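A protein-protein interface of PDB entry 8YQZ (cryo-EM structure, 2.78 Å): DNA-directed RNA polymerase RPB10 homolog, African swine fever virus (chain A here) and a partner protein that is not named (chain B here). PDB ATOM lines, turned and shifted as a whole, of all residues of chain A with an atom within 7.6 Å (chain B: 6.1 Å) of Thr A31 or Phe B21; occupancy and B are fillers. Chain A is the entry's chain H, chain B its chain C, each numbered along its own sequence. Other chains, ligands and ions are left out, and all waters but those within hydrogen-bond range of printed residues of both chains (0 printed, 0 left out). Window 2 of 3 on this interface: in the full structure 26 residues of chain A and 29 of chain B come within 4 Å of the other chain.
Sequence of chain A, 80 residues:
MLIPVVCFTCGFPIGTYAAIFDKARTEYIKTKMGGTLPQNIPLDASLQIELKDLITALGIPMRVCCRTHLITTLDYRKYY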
ATOM      1  N   ILE A  20     -10.920 -18.564   2.045  1.00  0.00           N
ATOM      2  CA  ILE A  20     -11.338 -19.748   1.308  1.00  0.00           C
ATOM      3  C   ILE A  20     -10.168 -20.701   1.149  1.00  0.00           C
ATOM      4  O   ILE A  20     -10.313 -21.913   1.318  1.00  0.00           O
ATOM      5  CB  ILE A  20     -11.936 -19.364  -0.057  1.00  0.00           C
ATOM      6  CG1 ILE A  20     -13.145 -18.458   0.108  1.00  0.00           C
ATOM      7  CG2 ILE A  20     -12.333 -20.596  -0.830  1.00  0.00           C
ATOM      8  CD1 ILE A  20     -13.524 -17.747  -1.153  1.00  0.00           C
ATOM      9  N   LYS A  23      -9.367 -22.567   4.592  1.00  0.00           N
ATOM     10  CA  LYS A  23     -10.330 -23.616   4.919  1.00  0.00           C
ATOM     11  C   LYS A  23     -10.257 -24.777   3.933  1.00  0.00           C
ATOM     12  O   LYS A  23     -10.300 -25.951   4.328  1.00  0.00           O
ATOM     13  CB  LYS A  23     -11.741 -23.051   4.956  1.00  0.00           C
ATOM     14  CG  LYS A  23     -12.290 -22.923   6.343  1.00  0.00           C
ATOM     15  CD  LYS A  23     -13.791 -22.807   6.293  1.00  0.00           C
ATOM     16  CE  LYS A  23     -14.414 -24.185   6.241  1.00  0.00           C
ATOM     17  NZ  LYS A  23     -14.756 -24.693   7.595  1.00  0.00           N
ATOM     18  N   ALA A  24     -10.163 -24.469   2.639  1.00  0.00           N
ATOM     19  CA  ALA A  24     -10.135 -25.512   1.626  1.00  0.00           C
ATOM     20  C   ALA A  24      -8.875 -26.354   1.738  1.00  0.00           C
ATOM     21  O   ALA A  24      -8.907 -27.565   1.517  1.00  0.00           O
ATOM     22  CB  ALA A  24     -10.254 -24.887   0.241  1.00  0.00           C
ATOM     23  N   ARG A  25      -7.750 -25.730   2.078  1.00  0.00           N
ATOM     24  CA  ARG A  25      -6.527 -26.485   2.287  1.00  0.00           C
ATOM     25  C   ARG A  25      -6.657 -27.414   3.480  1.00  0.00           C
ATOM     26  O   ARG A  25      -6.203 -28.561   3.435  1.00  0.00           O
ATOM     27  CB  ARG A  25      -5.345 -25.538   2.478  1.00  0.00           C
ATOM     28  CG  ARG A  25      -4.112 -26.240   2.979  1.00  0.00           C
ATOM     29  CD  ARG A  25      -2.956 -25.312   3.064  1.00  0.00           C
ATOM     30  NE  ARG A  25      -3.187 -24.233   4.009  1.00  0.00           N
ATOM     31  CZ  ARG A  25      -2.309 -23.277   4.271  1.00  0.00           C
ATOM     32  NH1 ARG A  25      -1.130 -23.243   3.676  1.00  0.00           N
ATOM     33  NH2 ARG A  25      -2.625 -22.328   5.143  1.00  0.00           N
ATOM     34  N   THR A  26      -7.271 -26.937   4.563  1.00  0.00           N
ATOM     35  CA  THR A  26      -7.503 -27.821   5.704  1.00  0.00           C
ATOM     36  C   THR A  26      -8.306 -29.050   5.290  1.00  0.00           C
ATOM     37  O   THR A  26      -7.915 -30.191   5.574  1.00  0.00           O
ATOM     38  CB  THR A  26      -8.222 -27.064   6.819  1.00  0.00           C
ATOM     39  OG1 THR A  26      -7.283 -26.246   7.521  1.00  0.00           O
ATOM     40  CG2 THR A  26      -8.834 -28.027   7.795  1.00  0.00           C
ATOM     41  N   GLU A  27      -9.419 -28.830   4.585  1.00  0.00           N
ATOM     42  CA  GLU A  27     -10.264 -29.945   4.157  1.00  0.00           C
ATOM     43  C   GLU A  27      -9.525 -30.893   3.220  1.00  0.00           C
ATOM     44  O   GLU A  27      -9.651 -32.116   3.333  1.00  0.00           O
ATOM     45  CB  GLU A  27     -11.524 -29.420   3.477  1.00  0.00           C
ATOM     46  CG  GLU A  27     -12.735 -29.288   4.380  1.00  0.00           C
ATOM     47  CD  GLU A  27     -12.487 -28.428   5.598  1.00  0.00           C
ATOM     48  OE1 GLU A  27     -12.202 -28.991   6.674  1.00  0.00           O
ATOM     49  OE2 GLU A  27     -12.601 -27.190   5.486  1.00  0.00           O
ATOM     50  N   TYR A  28      -8.761 -30.343   2.281  1.00  0.00           N
ATOM     51  CA  TYR A  28      -8.040 -31.152   1.306  1.00  0.00           C
ATOM     52  C   TYR A  28      -6.969 -32.017   1.961  1.00  0.00           C
ATOM     53  O   TYR A  28      -6.817 -33.197   1.626  1.00  0.00           O
ATOM     54  CB  TYR A  28      -7.422 -30.219   0.273  1.00  0.00           C
ATOM     55  CG  TYR A  28      -6.871 -30.885  -0.950  1.00  0.00           C
ATOM     56  CD1 TYR A  28      -7.696 -31.254  -1.989  1.00  0.00           C
ATOM     57  CD2 TYR A  28      -5.517 -31.117  -1.076  1.00  0.00           C
ATOM     58  CE1 TYR A  28      -7.191 -31.849  -3.107  1.00  0.00           C
ATOM     59  CE2 TYR A  28      -5.007 -31.712  -2.188  1.00  0.00           C
ATOM     60  CZ  TYR A  28      -5.846 -32.077  -3.204  1.00  0.00           C
ATOM     61  OH  TYR A  28      -5.339 -32.674  -4.328  1.00  0.00           O
ATOM     62  N   ILE A  29      -6.202 -31.444   2.885  1.00  0.00           N
ATOM     63  CA  ILE A  29      -5.182 -32.224   3.573  1.00  0.00           C
ATOM     64  C   ILE A  29      -5.824 -33.308   4.426  1.00  0.00           C
ATOM     65  O   ILE A  29      -5.324 -34.438   4.498  1.00  0.00           O
ATOM     66  CB  ILE A  29      -4.281 -31.303   4.407  1.00  0.00           C
ATOM     67  CG1 ILE A  29      -3.354 -30.513   3.493  1.00  0.00           C
ATOM     68  CG2 ILE A  29      -3.482 -32.104   5.400  1.00  0.00           C
ATOM     69  CD1 ILE A  29      -2.577 -29.465   4.209  1.00  0.00           C
ATOM     70  N   LYS A  30      -6.940 -32.990   5.085  1.00  0.00           N
ATOM     71  CA  LYS A  30      -7.639 -34.024   5.831  1.00  0.00           C
ATOM     72  C   LYS A  30      -8.104 -35.151   4.923  1.00  0.00           C
ATOM     73  O   LYS A  30      -7.984 -36.321   5.294  1.00  0.00           O
ATOM     74  CB  LYS A  30      -8.820 -33.415   6.580  1.00  0.00           C
ATOM     75  CG  LYS A  30      -9.685 -34.409   7.308  1.00  0.00           C
ATOM     76  CD  LYS A  30     -10.557 -33.700   8.323  1.00  0.00           C
ATOM     77  CE  LYS A  30     -11.913 -34.374   8.470  1.00  0.00           C
ATOM     78  NZ  LYS A  30     -12.427 -34.911   7.177  1.00  0.00           N
ATOM     79  N   THR A  31      -8.608 -34.825   3.736  1.00  0.00           N
ATOM     80  CA  THR A  31      -8.995 -35.862   2.788  1.00  0.00           C
ATOM     81  C   THR A  31      -7.804 -36.719   2.378  1.00  0.00           C
ATOM     82  O   THR A  31      -7.918 -37.945   2.293  1.00  0.00           O
ATOM     83  CB  THR A  31      -9.652 -35.228   1.564  1.00  0.00           C
ATOM     84  OG1 THR A  31     -11.046 -35.043   1.817  1.00  0.00           O
ATOM     85  CG2 THR A  31      -9.478 -36.099   0.340  1.00  0.00           C
ATOM     86  N   LYS A  32      -6.656 -36.100   2.128  1.00  0.00           N
ATOM     87  CA  LYS A  32      -5.469 -36.839   1.709  1.00  0.00           C
ATOM     88  C   LYS A  32      -4.892 -37.734   2.797  1.00  0.00           C
ATOM     89  O   LYS A  32      -4.357 -38.796   2.475  1.00  0.00           O
ATOM     90  CB  LYS A  32      -4.382 -35.878   1.231  1.00  0.00           C
ATOM     91  CG  LYS A  32      -4.669 -35.222  -0.100  1.00  0.00           C
ATOM     92  CD  LYS A  32      -4.690 -36.224  -1.222  1.00  0.00           C
ATOM     93  CE  LYS A  32      -5.716 -35.844  -2.259  1.00  0.00           C
ATOM     94  NZ  LYS A  32      -5.245 -36.151  -3.637  1.00  0.00           N
ATOM     95  N   MET A  33      -4.965 -37.335   4.066  1.00  0.00           N
ATOM     96  CA  MET A  33      -4.498 -38.183   5.159  1.00  0.00           C
ATOM     97  C   MET A  33      -5.524 -39.233   5.570  1.00  0.00           C
ATOM     98  O   MET A  33      -5.167 -40.389   5.803  1.00  0.00           O
ATOM     99  CB  MET A  33      -4.118 -37.327   6.372  1.00  0.00           C
ATOM    100  CG  MET A  33      -3.214 -36.147   6.062  1.00  0.00           C
ATOM    101  SD  MET A  33      -1.459 -36.534   5.990  1.00  0.00           S
ATOM    102  CE  MET A  33      -1.283 -37.130   4.314  1.00  0.00           C
ATOM    103  N   GLY A  34      -6.793 -38.853   5.673  1.00  0.00           N
ATOM    104  CA  GLY A  34      -7.839 -39.813   5.965  1.00  0.00           C
ATOM    105  C   GLY A  34      -8.206 -39.923   7.430  1.00  0.00           C
ATOM    106  O   GLY A  34      -8.260 -41.029   7.976  1.00  0.00           O
ATOM    107  N   GLY A  35      -8.445 -38.788   8.086  1.00  0.00           N
ATOM    108  CA  GLY A  35      -8.926 -38.805   9.455  1.00  0.00           C
ATOM    109  C   GLY A  35      -7.927 -39.299  10.485  1.00  0.00           C
ATOM    110  O   GLY A  35      -8.065 -40.412  11.002  1.00  0.00           O
ATOM    111  N   LEU A  54      -5.640 -26.541  -6.403  1.00  0.00           N
ATOM    112  CA  LEU A  54      -6.513 -25.787  -5.511  1.00  0.00           C
ATOM    113  C   LEU A  54      -6.332 -24.284  -5.703  1.00  0.00           C
ATOM    114  O   LEU A  54      -7.307 -23.526  -5.818  1.00  0.00           O
ATOM    115  CB  LEU A  54      -6.211 -26.189  -4.073  1.00  0.00           C
ATOM    116  CG  LEU A  54      -7.243 -26.089  -2.961  1.00  0.00           C
ATOM    117  CD1 LEU A  54      -8.336 -27.089  -3.171  1.00  0.00           C
ATOM    118  CD2 LEU A  54      -6.538 -26.337  -1.654  1.00  0.00           C
ATOM    119  N   ASN B  19     -14.568 -27.106  -8.428  1.00  0.00           N
ATOM    120  CA  ASN B  19     -13.754 -27.685  -7.371  1.00  0.00           C
ATOM    121  C   ASN B  19     -14.586 -27.750  -6.102  1.00  0.00           C
ATOM    122  O   ASN B  19     -15.115 -26.732  -5.650  1.00  0.00           O
ATOM    123  CB  ASN B  19     -12.487 -26.863  -7.155  1.00  0.00           C
ATOM    124  CG  ASN B  19     -11.490 -27.547  -6.249  1.00  0.00           C
ATOM    125  OD1 ASN B  19     -11.764 -27.782  -5.081  1.00  0.00           O
ATOM    126  ND2 ASN B  19     -10.327 -27.869  -6.783  1.00  0.00           N
ATOM    127  N   LEU B  20     -14.714 -28.945  -5.531  1.00  0.00           N
ATOM    128  CA  LEU B  20     -15.638 -29.135  -4.420  1.00  0.00           C
ATOM    129  C   LEU B  20     -15.156 -28.441  -3.156  1.00  0.00           C
ATOM    130  O   LEU B  20     -15.958 -27.859  -2.422  1.00  0.00           O
ATOM    131  CB  LEU B  20     -15.853 -30.623  -4.163  1.00  0.00           C
ATOM    132  CG  LEU B  20     -17.259 -31.119  -4.498  1.00  0.00           C
ATOM    133  CD1 LEU B  20     -17.542 -31.010  -5.987  1.00  0.00           C
ATOM    134  CD2 LEU B  20     -17.452 -32.540  -4.012  1.00  0.00           C
ATOM    135  N   PHE B  21     -13.859 -28.508  -2.873  1.00  0.00           N
ATOM    136  CA  PHE B  21     -13.339 -27.925  -1.643  1.00  0.00           C
ATOM    137  C   PHE B  21     -13.496 -26.409  -1.641  1.00  0.00           C
ATOM    138  O   PHE B  21     -13.908 -25.819  -0.635  1.00  0.00           O
ATOM    139  CB  PHE B  21     -11.881 -28.340  -1.468  1.00  0.00           C
ATOM    140  CG  PHE B  21     -11.680 -29.819  -1.507  1.00  0.00           C
ATOM    141  CD1 PHE B  21     -11.804 -30.576  -0.359  1.00  0.00           C
ATOM    142  CD2 PHE B  21     -11.393 -30.460  -2.693  1.00  0.00           C
ATOM    143  CE1 PHE B  21     -11.635 -31.935  -0.393  1.00  0.00           C
ATOM    144  CE2 PHE B  21     -11.221 -31.817  -2.730  1.00  0.00           C
ATOM    145  CZ  PHE B  21     -11.340 -32.555  -1.580  1.00  0.00           C
ATOM    146  N   ILE B  22     -13.191 -25.761  -2.770  1.00  0.00           N
ATOM    147  CA  ILE B  22     -13.393 -24.320  -2.886  1.00  0.00           C
ATOM    148  C   ILE B  22     -14.866 -23.981  -2.726  1.00  0.00           C
ATOM    149  O   ILE B  22     -15.226 -23.027  -2.029  1.00  0.00           O
ATOM    150  CB  ILE B  22     -12.841 -23.803  -4.229  1.00  0.00           C
ATOM    151  CG1 ILE B  22     -11.333 -24.027  -4.334  1.00  0.00           C
ATOM    152  CG2 ILE B  22     -13.156 -22.336  -4.401  1.00  0.00           C
ATOM    153  CD1 ILE B  22     -10.531 -23.317  -3.292  1.00  0.00           C
ATOM    154  N   LYS B  23     -15.743 -24.759  -3.361  1.00  0.00           N
ATOM    155  CA  LYS B  23     -17.174 -24.494  -3.275  1.00  0.00           C
ATOM    156  C   LYS B  23     -17.672 -24.591  -1.840  1.00  0.00           C
ATOM    157  O   LYS B  23     -18.420 -23.728  -1.370  1.00  0.00           O
ATOM    158  CB  LYS B  23     -17.940 -25.464  -4.170  1.00  0.00           C
ATOM    159  CG  LYS B  23     -19.367 -25.689  -3.728  1.00  0.00           C
ATOM    160  CD  LYS B  23     -20.181 -26.401  -4.783  1.00  0.00           C
ATOM    161  CE  LYS B  23     -20.464 -25.495  -5.966  1.00  0.00           C
ATOM    162  NZ  LYS B  23     -20.420 -26.237  -7.259  1.00  0.00           N
ATOM    163  N   ASN B  24     -17.265 -25.639  -1.127  1.00  0.00           N
ATOM    164  CA  ASN B  24     -17.729 -25.815   0.243  1.00  0.00           C
ATOM    165  C   ASN B  24     -17.199 -24.718   1.155  1.00  0.00           C
ATOM    166  O   ASN B  24     -17.951 -24.170   1.974  1.00  0.00           O
ATOM    167  CB  ASN B  24     -17.322 -27.192   0.761  1.00  0.00           C
ATOM    168  CG  ASN B  24     -17.988 -28.321   0.004  1.00  0.00           C
ATOM    169  OD1 ASN B  24     -19.099 -28.180  -0.491  1.00  0.00           O
ATOM    170  ND2 ASN B  24     -17.311 -29.453  -0.081  1.00  0.00           N
ATOM    171  N   ALA B  25     -15.916 -24.373   1.024  1.00  0.00           N
ATOM    172  CA  ALA B  25     -15.357 -23.315   1.859  1.00  0.00           C
ATOM    173  C   ALA B  25     -16.044 -21.983   1.597  1.00  0.00           C
ATOM    174  O   ALA B  25     -16.405 -21.266   2.537  1.00  0.00           O
ATOM    175  CB  ALA B  25     -13.856 -23.200   1.619  1.00  0.00           C
ATOM    176  N   ALA B  26     -16.256 -21.646   0.325  1.00  0.00           N
ATOM    177  CA  ALA B  26     -16.917 -20.394  -0.010  1.00  0.00           C
ATOM    178  C   ALA B  26     -18.339 -20.360   0.523  1.00  0.00           C
ATOM    179  O   ALA B  26     -18.763 -19.366   1.124  1.00  0.00           O
ATOM    180  CB  ALA B  26     -16.900 -20.196  -1.522  1.00  0.00           C
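Of the 15 printed residues of chain A, 6 touch a printed residue of chain B. Of the 8 printed residues of chain B, 4 touch a printed residue of chain A. Hydrophobic or aromatic side chains of chain B within 4 Å of the printed part of chain A: Phe B21, Ile B22 and Ala B25. Along chain B the printed residues that touch a printed residue of chain A span positions 19 to 25.
Of the printed residues of chain B, Ala A24 touches Phe B21 (3.9 Å) and Ile B22 (3.9 Å). Of chain B, only Phe B21 (3.9 Å) comes within 4 Å of Thr A31. Of the printed residues of chain A, Phe B21 touches Ala A24, Tyr A28 and Thr A31. Of the printed residues of chain A, Ala B25 touches Ile A20 (3.8 Å) and Lys A23 (3.95 Å). The nearest printed residue of chain A that does not touch Phe B21 is Glu A27 (4.02 Å). The nearest printed residue of chain B that does not touch Leu A54 is Ile B22 (4.1 Å).
NZ of Lys A23 lies within salt-bridge range of OE2 of Glu A27 (3.9 Å). OD1 of Asn B19 lies within hydrogen-bond range of N of Phe B21 (3.1 Å). OD1 of Asn B19 is in hydrogen-bond range of N of Ile B22 (3.4 Å).
Among the printed residues, pairs that only touch across the chains: Tyr A28 with Phe B21 (3.6 Å), Ile A20 with Ala B25 (3.8 Å), Thr A31 with Phe B21 (3.9 Å), Ala A24 with Phe B21 (3.9 Å), Ala A24 with Ile B22 (3.9 Å), Lys A23 with Ala B25 (3.95 Å), Ile A20 with Ile B22 (3.96 Å) and Leu A54 with Asn B19 (3.98 Å).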
